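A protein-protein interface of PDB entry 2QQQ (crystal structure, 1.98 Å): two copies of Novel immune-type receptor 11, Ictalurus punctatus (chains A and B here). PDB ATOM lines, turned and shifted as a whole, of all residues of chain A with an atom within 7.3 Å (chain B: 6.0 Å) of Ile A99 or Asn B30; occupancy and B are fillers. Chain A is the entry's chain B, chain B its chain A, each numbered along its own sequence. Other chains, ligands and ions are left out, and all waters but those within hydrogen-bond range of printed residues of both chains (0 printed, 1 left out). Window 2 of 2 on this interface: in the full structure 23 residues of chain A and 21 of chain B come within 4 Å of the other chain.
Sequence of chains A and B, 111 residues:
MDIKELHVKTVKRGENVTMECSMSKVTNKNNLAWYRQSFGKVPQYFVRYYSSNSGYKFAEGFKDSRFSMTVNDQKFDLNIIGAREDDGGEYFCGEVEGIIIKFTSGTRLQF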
ATOM      1  N   ASN A  31       1.971 -16.590   7.488  1.00  0.00           N
ATOM      2  CA  ASN A  31       3.360 -16.870   7.130  1.00  0.00           C
ATOM      3  C   ASN A  31       3.552 -18.286   6.565  1.00  0.00           C
ATOM      4  O   ASN A  31       4.634 -18.678   6.251  1.00  0.00           O
ATOM      5  CB  ASN A  31       4.240 -16.649   8.347  1.00  0.00           C
ATOM      6  CG  ASN A  31       4.893 -15.266   8.367  1.00  0.00           C
ATOM      7  OD1 ASN A  31       5.926 -15.059   9.022  1.00  0.00           O
ATOM      8  ND2 ASN A  31       4.313 -14.334   7.636  1.00  0.00           N
ATOM      9  N   VAL A  96       7.568 -19.103   7.391  1.00  0.00           N
ATOM     10  CA  VAL A  96       8.615 -18.101   7.621  1.00  0.00           C
ATOM     11  C   VAL A  96       8.587 -17.473   9.035  1.00  0.00           C
ATOM     12  O   VAL A  96       7.587 -16.864   9.446  1.00  0.00           O
ATOM     13  CB  VAL A  96       8.589 -16.965   6.558  1.00  0.00           C
ATOM     14  CG1 VAL A  96       9.532 -15.825   7.006  1.00  0.00           C
ATOM     15  CG2 VAL A  96       9.065 -17.530   5.249  1.00  0.00           C
ATOM     16  N   GLU A  97       9.676 -17.682   9.764  1.00  0.00           N
ATOM     17  CA  GLU A  97       9.950 -16.965  10.973  1.00  0.00           C
ATOM     18  C   GLU A  97      11.212 -16.086  10.836  1.00  0.00           C
ATOM     19  O   GLU A  97      12.340 -16.573  10.855  1.00  0.00           O
ATOM     20  CB  GLU A  97      10.058 -17.929  12.152  1.00  0.00           C
ATOM     21  CG  GLU A  97       8.784 -18.790  12.344  1.00  0.00           C
ATOM     22  CD  GLU A  97       9.024 -19.970  13.300  1.00  0.00           C
ATOM     23  OE1 GLU A  97       8.057 -20.418  13.996  1.00  0.00           O
ATOM     24  OE2 GLU A  97      10.194 -20.429  13.337  1.00  0.00           O
ATOM     25  N   GLY A  98      11.003 -14.779  10.729  1.00  0.00           N
ATOM     26  CA  GLY A  98      12.122 -13.851  10.694  1.00  0.00           C
ATOM     27  C   GLY A  98      13.169 -14.253   9.687  1.00  0.00           C
ATOM     28  O   GLY A  98      14.347 -14.604  10.052  1.00  0.00           O
ATOM     29  N   ILE A  99      12.746 -14.164   8.431  1.00  0.00           N
ATOM     30  CA  ILE A  99      13.523 -14.576   7.236  1.00  0.00           C
ATOM     31  C   ILE A  99      13.991 -16.034   7.068  1.00  0.00           C
ATOM     32  O   ILE A  99      14.519 -16.372   6.022  1.00  0.00           O
ATOM     33  CB  ILE A  99      14.673 -13.614   6.849  1.00  0.00           C
ATOM     34  CG1 ILE A  99      15.850 -13.720   7.837  1.00  0.00           C
ATOM     35  CG2 ILE A  99      14.119 -12.202   6.655  1.00  0.00           C
ATOM     36  CD1 ILE A  99      17.127 -13.015   7.391  1.00  0.00           C
ATOM     37  N   ILE A 100      13.845 -16.874   8.087  1.00  0.00           N
ATOM     38  CA  ILE A 100      14.126 -18.274   7.939  1.00  0.00           C
ATOM     39  C   ILE A 100      12.812 -19.015   7.700  1.00  0.00           C
ATOM     40  O   ILE A 100      11.851 -18.863   8.489  1.00  0.00           O
ATOM     41  CB  ILE A 100      14.838 -18.840   9.181  1.00  0.00           C
ATOM     42  CG1 ILE A 100      16.224 -18.238   9.302  1.00  0.00           C
ATOM     43  CG2 ILE A 100      14.979 -20.360   9.100  1.00  0.00           C
ATOM     44  CD1 ILE A 100      17.006 -18.147   8.044  1.00  0.00           C
ATOM     45  N   ILE A 101      12.748 -19.832   6.636  1.00  0.00           N
ATOM     46  CA  ILE A 101      11.572 -20.664   6.417  1.00  0.00           C
ATOM     47  C   ILE A 101      11.805 -22.009   7.142  1.00  0.00           C
ATOM     48  O   ILE A 101      12.844 -22.585   7.002  1.00  0.00           O
ATOM     49  CB  ILE A 101      11.225 -20.800   4.876  1.00  0.00           C
ATOM     50  CG1 ILE A 101       9.874 -21.488   4.629  1.00  0.00           C
ATOM     51  CG2 ILE A 101      12.285 -21.456   4.072  1.00  0.00           C
ATOM     52  CD1 ILE A 101       9.721 -22.951   5.101  1.00  0.00           C
ATOM     53  N   LYS A 102      10.862 -22.461   7.974  1.00  0.00           N
ATOM     54  CA  LYS A 102      10.947 -23.802   8.553  1.00  0.00           C
ATOM     55  C   LYS A 102       9.923 -24.647   7.879  1.00  0.00           C
ATOM     56  O   LYS A 102       8.736 -24.291   7.884  1.00  0.00           O
ATOM     57  CB  LYS A 102      10.618 -23.807  10.047  1.00  0.00           C
ATOM     58  CG  LYS A 102      11.751 -23.497  10.942  1.00  0.00           C
ATOM     59  CD  LYS A 102      12.667 -24.731  11.178  1.00  0.00           C
ATOM     60  CE  LYS A 102      14.028 -24.356  11.824  1.00  0.00           C
ATOM     61  NZ  LYS A 102      13.877 -23.419  13.006  1.00  0.00           N
ATOM     62  N   ASN B  28      19.044  -8.184  -1.374  1.00  0.00           N
ATOM     63  CA  ASN B  28      19.388  -7.980  -0.010  1.00  0.00           C
ATOM     64  C   ASN B  28      20.196  -9.209   0.504  1.00  0.00           C
ATOM     65  O   ASN B  28      19.634 -10.229   0.933  1.00  0.00           O
ATOM     66  CB  ASN B  28      18.096  -7.675   0.777  1.00  0.00           C
ATOM     67  CG  ASN B  28      18.293  -7.587   2.284  1.00  0.00           C
ATOM     68  OD1 ASN B  28      19.344  -7.183   2.788  1.00  0.00           O
ATOM     69  ND2 ASN B  28      17.252  -7.955   3.017  1.00  0.00           N
ATOM     70  N   LYS B  29      21.531  -9.090   0.430  1.00  0.00           N
ATOM     71  CA  LYS B  29      22.451 -10.059   1.029  1.00  0.00           C
ATOM     72  C   LYS B  29      22.016 -10.520   2.432  1.00  0.00           C
ATOM     73  O   LYS B  29      22.058 -11.698   2.772  1.00  0.00           O
ATOM     74  CB  LYS B  29      23.857  -9.471   1.068  1.00  0.00           C
ATOM     75  CG  LYS B  29      24.443  -9.297  -0.317  1.00  0.00           C
ATOM     76  CD  LYS B  29      25.761  -8.516  -0.300  1.00  0.00           C
ATOM     77  CE  LYS B  29      26.169  -8.225  -1.737  1.00  0.00           C
ATOM     78  NZ  LYS B  29      27.682  -8.065  -1.877  1.00  0.00           N
ATOM     79  N   ASN B  30      21.560  -9.573   3.231  1.00  0.00           N
ATOM     80  CA  ASN B  30      21.168  -9.860   4.598  1.00  0.00           C
ATOM     81  C   ASN B  30      20.070 -10.908   4.671  1.00  0.00           C
ATOM     82  O   ASN B  30      19.796 -11.433   5.732  1.00  0.00           O
ATOM     83  CB  ASN B  30      20.671  -8.589   5.275  1.00  0.00           C
ATOM     84  CG  ASN B  30      21.756  -7.560   5.457  1.00  0.00           C
ATOM     85  OD1 ASN B  30      21.487  -6.370   5.303  1.00  0.00           O
ATOM     86  ND2 ASN B  30      22.992  -8.000   5.743  1.00  0.00           N
ATOM     87  N   ASN B  31      19.436 -11.173   3.537  1.00  0.00           N
ATOM     88  CA  ASN B  31      18.312 -12.073   3.480  1.00  0.00           C
ATOM     89  C   ASN B  31      18.623 -13.322   2.674  1.00  0.00           C
ATOM     90  O   ASN B  31      17.722 -14.101   2.388  1.00  0.00           O
ATOM     91  CB  ASN B  31      17.056 -11.350   2.959  1.00  0.00           C
ATOM     92  CG  ASN B  31      16.347 -10.496   4.024  1.00  0.00           C
ATOM     93  OD1 ASN B  31      15.248  -9.973   3.769  1.00  0.00           O
ATOM     94  ND2 ASN B  31      16.941 -10.343   5.185  1.00  0.00           N
ATOM     95  N   LEU B  32      19.908 -13.522   2.346  1.00  0.00           N
ATOM     96  CA  LEU B  32      20.369 -14.626   1.515  1.00  0.00           C
ATOM     97  C   LEU B  32      20.830 -15.789   2.389  1.00  0.00           C
ATOM     98  O   LEU B  32      21.431 -15.571   3.433  1.00  0.00           O
ATOM     99  CB  LEU B  32      21.567 -14.171   0.664  1.00  0.00           C
ATOM    100  CG  LEU B  32      22.131 -15.076  -0.424  1.00  0.00           C
ATOM    101  CD1 LEU B  32      21.166 -15.223  -1.581  1.00  0.00           C
ATOM    102  CD2 LEU B  32      23.447 -14.448  -0.954  1.00  0.00           C
ATOM    103  N   TYR B  35      19.826 -23.548   1.856  1.00  0.00           N
ATOM    104  CA  TYR B  35      18.973 -24.636   2.455  1.00  0.00           C
ATOM    105  C   TYR B  35      19.531 -25.975   1.931  1.00  0.00           C
ATOM    106  O   TYR B  35      20.071 -26.065   0.808  1.00  0.00           O
ATOM    107  CB  TYR B  35      17.473 -24.419   2.059  1.00  0.00           C
ATOM    108  CG  TYR B  35      16.913 -23.220   2.800  1.00  0.00           C
ATOM    109  CD1 TYR B  35      17.234 -21.886   2.439  1.00  0.00           C
ATOM    110  CD2 TYR B  35      16.006 -23.408   3.854  1.00  0.00           C
ATOM    111  CE1 TYR B  35      16.722 -20.800   3.188  1.00  0.00           C
ATOM    112  CE2 TYR B  35      15.534 -22.374   4.578  1.00  0.00           C
ATOM    113  CZ  TYR B  35      15.893 -21.071   4.271  1.00  0.00           C
ATOM    114  OH  TYR B  35      15.367 -20.098   5.078  1.00  0.00           O
ATOM    115  N   ARG B  48      23.478 -18.667   6.622  1.00  0.00           N
ATOM    116  CA  ARG B  48      23.097 -17.393   6.059  1.00  0.00           C
ATOM    117  C   ARG B  48      24.310 -16.469   5.858  1.00  0.00           C
ATOM    118  O   ARG B  48      25.320 -16.594   6.557  1.00  0.00           O
ATOM    119  CB  ARG B  48      22.081 -16.746   6.966  1.00  0.00           C
ATOM    120  CG  ARG B  48      22.636 -16.275   8.287  1.00  0.00           C
ATOM    121  CD  ARG B  48      21.586 -15.395   8.854  1.00  0.00           C
ATOM    122  NE  ARG B  48      21.998 -14.798  10.108  1.00  0.00           N
ATOM    123  CZ  ARG B  48      21.201 -14.073  10.880  1.00  0.00           C
ATOM    124  NH1 ARG B  48      19.913 -13.858  10.513  1.00  0.00           N
ATOM    125  NH2 ARG B  48      21.684 -13.600  12.033  1.00  0.00           N
ATOM    126  N   TYR B  49      24.194 -15.567   4.886  1.00  0.00           N
ATOM    127  CA  TYR B  49      24.999 -14.363   4.848  1.00  0.00           C
ATOM    128  C   TYR B  49      24.851 -13.606   6.183  1.00  0.00           C
ATOM    129  O   TYR B  49      23.759 -13.481   6.748  1.00  0.00           O
ATOM    130  CB  TYR B  49      24.571 -13.452   3.703  1.00  0.00           C
ATOM    131  CG  TYR B  49      25.466 -12.248   3.510  1.00  0.00           C
ATOM    132  CD1 TYR B  49      25.341 -11.109   4.332  1.00  0.00           C
ATOM    133  CD2 TYR B  49      26.461 -12.251   2.525  1.00  0.00           C
ATOM    134  CE1 TYR B  49      26.181 -10.012   4.159  1.00  0.00           C
ATOM    135  CE2 TYR B  49      27.308 -11.140   2.344  1.00  0.00           C
ATOM    136  CZ  TYR B  49      27.134 -10.022   3.147  1.00  0.00           C
ATOM    137  OH  TYR B  49      27.952  -8.927   2.979  1.00  0.00           O
ATOM    138  N   TYR B  50      25.982 -13.118   6.669  1.00  0.00           N
ATOM    139  CA  TYR B  50      26.129 -12.539   7.973  1.00  0.00           C
ATOM    140  C   TYR B  50      27.318 -11.551   8.002  1.00  0.00           C
ATOM    141  O   TYR B  50      28.459 -11.982   8.106  1.00  0.00           O
ATOM    142  CB  TYR B  50      26.282 -13.693   9.023  1.00  0.00           C
ATOM    143  CG  TYR B  50      26.328 -13.246  10.449  1.00  0.00           C
ATOM    144  CD1 TYR B  50      25.156 -12.979  11.143  1.00  0.00           C
ATOM    145  CD2 TYR B  50      27.570 -13.115  11.121  1.00  0.00           C
ATOM    146  CE1 TYR B  50      25.204 -12.566  12.498  1.00  0.00           C
ATOM    147  CE2 TYR B  50      27.635 -12.707  12.467  1.00  0.00           C
ATOM    148  CZ  TYR B  50      26.416 -12.444  13.143  1.00  0.00           C
ATOM    149  OH  TYR B  50      26.413 -12.060  14.456  1.00  0.00           O
ATOM    150  N   SER B  51      27.036 -10.235   7.956  1.00  0.00           N
ATOM    151  CA  SER B  51      28.116  -9.237   8.020  1.00  0.00           C
ATOM    152  C   SER B  51      28.970  -9.397   9.236  1.00  0.00           C
ATOM    153  O   SER B  51      28.506  -9.245  10.377  1.00  0.00           O
ATOM    154  CB  SER B  51      27.618  -7.784   7.989  1.00  0.00           C
ATOM    155  OG  SER B  51      26.787  -7.660   6.894  1.00  0.00           O
ATOM    156  N   VAL B  96      15.128 -14.180   0.889  1.00  0.00           N
ATOM    157  CA  VAL B  96      13.778 -13.807   1.341  1.00  0.00           C
ATOM    158  C   VAL B  96      13.397 -12.354   1.061  1.00  0.00           C
ATOM    159  O   VAL B  96      14.184 -11.436   1.323  1.00  0.00           O
ATOM    160  CB  VAL B  96      13.532 -14.082   2.806  1.00  0.00           C
ATOM    161  CG1 VAL B  96      12.151 -13.583   3.202  1.00  0.00           C
ATOM    162  CG2 VAL B  96      13.697 -15.602   3.063  1.00  0.00           C
ATOM    163  N   GLY B  98       9.978 -10.150   1.858  1.00  0.00           N
ATOM    164  CA  GLY B  98       8.672 -10.147   2.463  1.00  0.00           C
ATOM    165  C   GLY B  98       8.576 -11.471   3.182  1.00  0.00           C
ATOM    166  O   GLY B  98       9.247 -11.688   4.182  1.00  0.00           O
ATOM    167  N   ILE B 101      10.459 -16.864   0.091  1.00  0.00           N
ATOM    168  CA  ILE B 101      11.821 -17.215  -0.249  1.00  0.00           C
ATOM    169  C   ILE B 101      11.836 -17.521  -1.739  1.00  0.00           C
ATOM    170  O   ILE B 101      11.062 -18.360  -2.212  1.00  0.00           O
ATOM    171  CB  ILE B 101      12.340 -18.402   0.683  1.00  0.00           C
ATOM    172  CG1 ILE B 101      13.851 -18.309   1.040  1.00  0.00           C
ATOM    173  CG2 ILE B 101      11.770 -19.776   0.280  1.00  0.00           C
ATOM    174  CD1 ILE B 101      14.761 -18.581  -0.109  1.00  0.00           C
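The backbone NH (N) of Ile A101 sits at hydrogen-bond distance from the side-chain hydroxyl (OH) of Tyr B35, 3.1 Å away.
OD1 of Asn B28 sits close to N of Asn B30 (3.3 Å).
OD1 of Asn B31 lies close to ND2 of Asn B28 (2.9 Å).
The backbone carbonyl oxygen (O) of Asn B31 is in hydrogen-bond range of the backbone NH (N) of Val B96 (3.0 Å).
Among the printed residues, pairs that only touch across the chains: Ile A99 with Val B96 (3.2 Å), Ile A99 with Asn B31 (3.5 Å), Ile A99 with Asn B30 (3.5 Å), Ile A100 with Tyr B35 (3.6 Å) and Ile A99 with Tyr B35 (3.9 Å).
Ile A99 touches just these residues of chain B: Asn B30 (3.5 Å), Asn B31 (3.5 Å), Tyr B35 (3.9 Å) and Val B96 (3.2 Å).
Printed residues of chain A within 4 Å of Asn B30: Ile A99.
Printed residues of chain A within 4 Å of Val B96: Ile A99 (3.2 Å).
Printed residues of chain A within 4 Å of Asn B31: Ile A99 (3.5 Å).
Gly B98 touches none of the printed residues of chain A.
The nearest residue of chain B that does not touch Ile A99 is Arg B48 (4.3 Å).
The nearest printed residue of chain A that does not touch Tyr B35 is Lys A102 (5.8 Å).
Hydrophobic or aromatic side chains of chain A that line the printed part of chain B: Ile A99, Ile A100 and Ile A101.
Printed residues of chain B that touch a printed residue of chain A: Asn B30, Asn B31, Tyr B35 and Val B96.
Among the printed residues, 6 pairs touch across the chains.
4 positions are printed for both chains.
Of the 6 pairs that touch across the chains among the printed residues, none has its exchanged pair printed and touching as well.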
